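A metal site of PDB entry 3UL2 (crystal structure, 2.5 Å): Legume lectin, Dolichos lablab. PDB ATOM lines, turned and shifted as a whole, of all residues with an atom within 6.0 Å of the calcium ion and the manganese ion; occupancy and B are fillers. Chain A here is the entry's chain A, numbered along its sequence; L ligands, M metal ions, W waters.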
ATOM      1  N   ASP A 108       9.051  29.017 -19.042  1.00  0.00           N
ATOM      2  CA  ASP A 108       9.215  27.770 -19.774  1.00  0.00           C
ATOM      3  C   ASP A 108       7.993  27.405 -20.601  1.00  0.00           C
ATOM      4  O   ASP A 108       8.117  26.759 -21.642  1.00  0.00           O
ATOM      5  CB  ASP A 108       9.546  26.631 -18.803  1.00  0.00           C
ATOM      6  CG  ASP A 108      11.029  26.429 -18.639  1.00  0.00           C
ATOM      7  OD1 ASP A 108      11.636  25.786 -19.510  1.00  0.00           O
ATOM      8  OD2 ASP A 108      11.579  26.906 -17.640  1.00  0.00           O
ATOM      9  N   GLY A 126      11.575  23.477 -17.048  1.00  0.00           N
ATOM     10  CA  GLY A 126      11.168  22.765 -18.262  1.00  0.00           C
ATOM     11  C   GLY A 126      10.184  21.616 -18.058  1.00  0.00           C
ATOM     12  O   GLY A 126       9.556  21.171 -19.018  1.00  0.00           O
ATOM     13  N   LEU A 128       7.552  21.966 -16.266  1.00  0.00           N
ATOM     14  CA  LEU A 128       6.266  22.662 -16.238  1.00  0.00           C
ATOM     15  C   LEU A 128       5.402  22.405 -14.997  1.00  0.00           C
ATOM     16  O   LEU A 128       4.205  22.683 -15.003  1.00  0.00           O
ATOM     17  CB  LEU A 128       5.473  22.373 -17.535  1.00  0.00           C
ATOM     18  CG  LEU A 128       6.169  22.683 -18.868  1.00  0.00           C
ATOM     19  CD1 LEU A 128       5.405  22.067 -20.031  1.00  0.00           C
ATOM     20  CD2 LEU A 128       6.351  24.186 -19.068  1.00  0.00           C
ATOM     21  N   GLU A 146       0.788  20.701 -23.689  1.00  0.00           N
ATOM     22  CA  GLU A 146       1.744  21.744 -23.341  1.00  0.00           C
ATOM     23  C   GLU A 146       1.879  22.774 -24.453  1.00  0.00           C
ATOM     24  O   GLU A 146       1.707  22.468 -25.642  1.00  0.00           O
ATOM     25  CB  GLU A 146       3.113  21.156 -22.991  1.00  0.00           C
ATOM     26  CG  GLU A 146       3.786  20.394 -24.130  1.00  0.00           C
ATOM     27  CD  GLU A 146       5.235  20.050 -23.838  1.00  0.00           C
ATOM     28  OE1 GLU A 146       5.543  19.627 -22.712  1.00  0.00           O
ATOM     29  OE2 GLU A 146       6.062  20.216 -24.755  1.00  0.00           O
ATOM     30  N   ASP A 148       4.900  25.045 -25.179  1.00  0.00           N
ATOM     31  CA  ASP A 148       6.282  25.037 -24.703  1.00  0.00           C
ATOM     32  C   ASP A 148       7.118  26.142 -25.366  1.00  0.00           C
ATOM     33  O   ASP A 148       7.467  26.044 -26.541  1.00  0.00           O
ATOM     34  CB  ASP A 148       6.875  23.655 -24.960  1.00  0.00           C
ATOM     35  CG  ASP A 148       8.164  23.413 -24.181  1.00  0.00           C
ATOM     36  OD1 ASP A 148       8.825  24.388 -23.760  1.00  0.00           O
ATOM     37  OD2 ASP A 148       8.513  22.219 -23.993  1.00  0.00           O
ATOM     38  N   THR A 149       7.441  27.153 -24.562  1.00  0.00           N
ATOM     39  CA  THR A 149       8.143  28.361 -25.024  1.00  0.00           C
ATOM     40  C   THR A 149       9.659  28.176 -25.077  1.00  0.00           C
ATOM     41  O   THR A 149      10.367  29.031 -25.607  1.00  0.00           O
ATOM     42  CB  THR A 149       7.892  29.560 -24.059  1.00  0.00           C
ATOM     43  OG1 THR A 149       6.487  29.869 -24.006  1.00  0.00           O
ATOM     44  CG2 THR A 149       8.670  30.793 -24.480  1.00  0.00           C
ATOM     45  N   PHE A 150      10.158  27.071 -24.531  1.00  0.00           N
ATOM     46  CA  PHE A 150      11.608  26.915 -24.352  1.00  0.00           C
ATOM     47  C   PHE A 150      12.197  25.583 -24.799  1.00  0.00           C
ATOM     48  O   PHE A 150      11.724  24.515 -24.418  1.00  0.00           O
ATOM     49  CB  PHE A 150      12.005  27.200 -22.890  1.00  0.00           C
ATOM     50  CG  PHE A 150      13.493  27.198 -22.665  1.00  0.00           C
ATOM     51  CD1 PHE A 150      14.151  26.026 -22.306  1.00  0.00           C
ATOM     52  CD2 PHE A 150      14.231  28.354 -22.827  1.00  0.00           C
ATOM     53  CE1 PHE A 150      15.515  26.005 -22.103  1.00  0.00           C
ATOM     54  CE2 PHE A 150      15.590  28.353 -22.618  1.00  0.00           C
ATOM     55  CZ  PHE A 150      16.238  27.172 -22.255  1.00  0.00           C
ATOM     56  N   TYR A 151      13.291  25.676 -25.557  1.00  0.00           N
ATOM     57  CA  TYR A 151      14.004  24.534 -26.131  1.00  0.00           C
ATOM     58  C   TYR A 151      14.830  23.825 -25.063  1.00  0.00           C
ATOM     59  O   TYR A 151      15.934  24.247 -24.744  1.00  0.00           O
ATOM     60  CB  TYR A 151      14.876  25.049 -27.280  1.00  0.00           C
ATOM     61  CG  TYR A 151      15.670  24.038 -28.095  1.00  0.00           C
ATOM     62  CD1 TYR A 151      15.196  22.757 -28.321  1.00  0.00           C
ATOM     63  CD2 TYR A 151      16.877  24.408 -28.690  1.00  0.00           C
ATOM     64  CE1 TYR A 151      15.923  21.846 -29.092  1.00  0.00           C
ATOM     65  CE2 TYR A 151      17.609  23.527 -29.461  1.00  0.00           C
ATOM     66  CZ  TYR A 151      17.128  22.246 -29.659  1.00  0.00           C
ATOM     67  OH  TYR A 151      17.859  21.354 -30.430  1.00  0.00           O
ATOM     68  N   ASN A 152      14.271  22.752 -24.514  1.00  0.00           N
ATOM     69  CA  ASN A 152      14.978  21.955 -23.505  1.00  0.00           C
ATOM     70  C   ASN A 152      15.859  20.857 -24.103  1.00  0.00           C
ATOM     71  O   ASN A 152      16.655  20.243 -23.391  1.00  0.00           O
ATOM     72  CB  ASN A 152      14.005  21.342 -22.499  1.00  0.00           C
ATOM     73  CG  ASN A 152      13.583  22.319 -21.418  1.00  0.00           C
ATOM     74  OD1 ASN A 152      12.485  22.866 -21.455  1.00  0.00           O
ATOM     75  ND2 ASN A 152      14.458  22.541 -20.452  1.00  0.00           N
ATOM     76  N   TRP A 155      14.932  16.804 -24.604  1.00  0.00           N
ATOM     77  CA  TRP A 155      13.717  16.133 -25.047  1.00  0.00           C
ATOM     78  C   TRP A 155      12.901  16.920 -26.097  1.00  0.00           C
ATOM     79  O   TRP A 155      12.064  16.333 -26.789  1.00  0.00           O
ATOM     80  CB  TRP A 155      12.831  15.780 -23.841  1.00  0.00           C
ATOM     81  CG  TRP A 155      12.438  16.946 -22.985  1.00  0.00           C
ATOM     82  CD1 TRP A 155      11.370  17.771 -23.186  1.00  0.00           C
ATOM     83  CD2 TRP A 155      13.085  17.407 -21.787  1.00  0.00           C
ATOM     84  NE1 TRP A 155      11.310  18.724 -22.184  1.00  0.00           N
ATOM     85  CE2 TRP A 155      12.349  18.518 -21.321  1.00  0.00           C
ATOM     86  CE3 TRP A 155      14.208  16.982 -21.066  1.00  0.00           C
ATOM     87  CZ2 TRP A 155      12.698  19.212 -20.157  1.00  0.00           C
ATOM     88  CZ3 TRP A 155      14.567  17.685 -19.907  1.00  0.00           C
ATOM     89  CH2 TRP A 155      13.813  18.781 -19.467  1.00  0.00           C
ATOM     90  N   ASP A 156      13.153  18.225 -26.216  1.00  0.00           N
ATOM     91  CA  ASP A 156      12.312  19.105 -27.038  1.00  0.00           C
ATOM     92  C   ASP A 156      12.682  19.162 -28.520  1.00  0.00           C
ATOM     93  O   ASP A 156      13.834  18.952 -28.888  1.00  0.00           O
ATOM     94  CB  ASP A 156      12.321  20.525 -26.466  1.00  0.00           C
ATOM     95  CG  ASP A 156      11.325  20.701 -25.339  1.00  0.00           C
ATOM     96  OD1 ASP A 156      10.328  19.948 -25.279  1.00  0.00           O
ATOM     97  OD2 ASP A 156      11.531  21.619 -24.513  1.00  0.00           O
ATOM     98  N   PRO A 157      11.679  19.453 -29.380  1.00  0.00           N
ATOM     99  CA  PRO A 157      11.960  19.844 -30.770  1.00  0.00           C
ATOM    100  C   PRO A 157      12.631  21.217 -30.801  1.00  0.00           C
ATOM    101  O   PRO A 157      12.663  21.910 -29.788  1.00  0.00           O
ATOM    102  CB  PRO A 157      10.566  19.924 -31.416  1.00  0.00           C
ATOM    103  CG  PRO A 157       9.650  19.194 -30.484  1.00  0.00           C
ATOM    104  CD  PRO A 157      10.233  19.393 -29.124  1.00  0.00           C
ATOM    105  N   HIS A 161       6.613  24.859 -29.545  1.00  0.00           N
ATOM    106  CA  HIS A 161       5.745  23.774 -29.952  1.00  0.00           C
ATOM    107  C   HIS A 161       4.550  23.578 -29.032  1.00  0.00           C
ATOM    108  O   HIS A 161       4.568  23.960 -27.858  1.00  0.00           O
ATOM    109  CB  HIS A 161       6.538  22.473 -30.058  1.00  0.00           C
ATOM    110  CG  HIS A 161       7.279  22.104 -28.818  1.00  0.00           C
ATOM    111  ND1 HIS A 161       8.475  22.681 -28.460  1.00  0.00           N
ATOM    112  CD2 HIS A 161       6.986  21.208 -27.837  1.00  0.00           C
ATOM    113  CE1 HIS A 161       8.895  22.166 -27.307  1.00  0.00           C
ATOM    114  NE2 HIS A 161       8.013  21.266 -26.915  1.00  0.00           N
ATOM    115  N   ASP A 165       1.527  15.398 -23.752  1.00  0.00           N
ATOM    116  CA  ASP A 165       2.341  14.755 -22.738  1.00  0.00           C
ATOM    117  C   ASP A 165       1.589  13.653 -21.995  1.00  0.00           C
ATOM    118  O   ASP A 165       0.569  13.908 -21.347  1.00  0.00           O
ATOM    119  CB  ASP A 165       2.833  15.799 -21.724  1.00  0.00           C
ATOM    120  CG  ASP A 165       3.713  16.874 -22.348  1.00  0.00           C
ATOM    121  OD1 ASP A 165       4.086  16.763 -23.539  1.00  0.00           O
ATOM    122  OD2 ASP A 165       4.032  17.850 -21.640  1.00  0.00           O
ATOM    123  N   ILE A 169       7.482  14.412 -19.685  1.00  0.00           N
ATOM    124  CA  ILE A 169       7.705  15.736 -20.277  1.00  0.00           C
ATOM    125  C   ILE A 169       8.113  15.603 -21.751  1.00  0.00           C
ATOM    126  O   ILE A 169       8.050  16.567 -22.520  1.00  0.00           O
ATOM    127  CB  ILE A 169       8.727  16.602 -19.478  1.00  0.00           C
ATOM    128  CG1 ILE A 169       8.667  18.074 -19.890  1.00  0.00           C
ATOM    129  CG2 ILE A 169      10.153  16.071 -19.623  1.00  0.00           C
ATOM    130  CD1 ILE A 169       7.366  18.779 -19.582  1.00  0.00           C
ATOM    131  N   SER A 171       7.064  14.766 -24.974  1.00  0.00           N
ATOM    132  CA  SER A 171       5.797  14.626 -25.693  1.00  0.00           C
ATOM    133  C   SER A 171       5.786  13.417 -26.620  1.00  0.00           C
ATOM    134  O   SER A 171       6.798  13.101 -27.250  1.00  0.00           O
ATOM    135  CB  SER A 171       5.514  15.891 -26.498  1.00  0.00           C
ATOM    136  OG  SER A 171       5.552  17.050 -25.689  1.00  0.00           O
ATOM    137  N   THR A 174       4.331  16.270 -31.231  1.00  0.00           N
ATOM    138  CA  THR A 174       4.355  17.734 -31.179  1.00  0.00           C
ATOM    139  C   THR A 174       3.971  18.344 -32.526  1.00  0.00           C
ATOM    140  O   THR A 174       3.853  17.625 -33.538  1.00  0.00           O
ATOM    141  CB  THR A 174       5.755  18.306 -30.779  1.00  0.00           C
ATOM    142  OG1 THR A 174       6.724  17.986 -31.783  1.00  0.00           O
ATOM    143  CG2 THR A 174       6.227  17.783 -29.424  1.00  0.00           C
HETATM  144  C1  LIG L   1      17.323  25.599 -17.465  1.00  0.00           C
HETATM  145  C2  LIG L   1      16.005  24.823 -17.498  1.00  0.00           C
HETATM  146  C3  LIG L   1      15.109  25.333 -18.636  1.00  0.00           C
HETATM  147  C4  LIG L   1      14.978  26.855 -18.599  1.00  0.00           C
HETATM  148  C5  LIG L   1      16.383  27.464 -18.561  1.00  0.00           C
HETATM  149  C6  LIG L   1      16.366  28.990 -18.569  1.00  0.00           C
HETATM  150  O1  LIG L   1      18.033  25.249 -16.297  1.00  0.00           O
HETATM  151  O2  LIG L   1      16.248  23.441 -17.651  1.00  0.00           O
HETATM  152  O3  LIG L   1      13.829  24.727 -18.549  1.00  0.00           O
HETATM  153  O4  LIG L   1      14.246  27.262 -17.478  1.00  0.00           O
HETATM  154  O5  LIG L   1      17.071  26.988 -17.423  1.00  0.00           O
HETATM  155  O6  LIG L   1      17.690  29.439 -18.706  1.00  0.00           O
HETATM  156 CA    CA M   1      10.750  22.963 -22.905  1.00  0.00          CA
HETATM  157 MN    MN M   2       8.276  20.202 -25.036  1.00  0.00          MN
HETATM  158  O   HOH W   1      10.183  24.396 -21.353  1.00  0.00           O
HETATM  159  O   HOH W   2       9.668  21.082 -21.765  1.00  0.00           O
HETATM  160  O   HOH W   3       7.781  18.593 -26.297  1.00  0.00           O
HETATM  161  O   HOH W   4       8.296  19.311 -22.996  1.00  0.00           O
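The nearest printed residue that does not touch the calcium ion is Trp 155 (4.3 Å).
Water W1 binds the calcium ion (2.2 Å). OD2 of Asp 156 binds the calcium ion (2.2 Å). OD1 of Asn 152 binds the calcium ion, at 2.3 Å. The backbone carbonyl oxygen (O) of Phe 150 is bound to the calcium ion, 2.4 Å away. The calcium ion is bound by water W2 (2.5 Å). The side-chain carboxylate (OD1) of Asp 148 is bound to the calcium ion (2.5 Å). OD2 of Asp 148 is bound to the calcium ion (2.6 Å). The calcium ion has seven donor atoms within binding distance.
OD1 of Asp 156 is bound to the manganese ion (2.1 Å). The manganese ion is bound by water W3 (2.1 Å). The manganese ion is bound by a ring nitrogen (NE2) of His 161 (2.2 Å). Water W4 binds the manganese ion, at 2.2 Å. The side-chain carboxylate (OE2) of Glu 146 is bound to the manganese ion, at 2.2 Å. OD2 of Asp 148 binds the manganese ion.
OG of Ser 171 lies close to OE2 of Glu 146. OE1 of Glu 146 sits close to OD2 of Asp 165, at 2.6 Å. NE1 of Trp 155 sits close to OD1 of Asp 156.
Water W2 bridges O of Gly 126 (2.8 Å) and NE1 of Trp 155 (2.9 Å). Water W4 lies within hydrogen-bond range of OE1 of Glu 146 (2.8 Å), O of Ile 169 (2.8 Å) and NE1 of Trp 155 (3.2 Å).
Within 4 Å of the manganese ion: Glu 146, Asp 148, Asp 156 and His 161.
O3 of the ligand sits at hydrogen-bond distance from N of Gly 126 (3.0 Å). An oxygen (O3) of the ligand is in hydrogen-bond range of the side-chain carboxylate (OD1) of Asp 108. The side-chain amide nitrogen (ND2) of Asn 152 lies within hydrogen-bond range of an oxygen (O3) of the ligand (3.0 Å).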
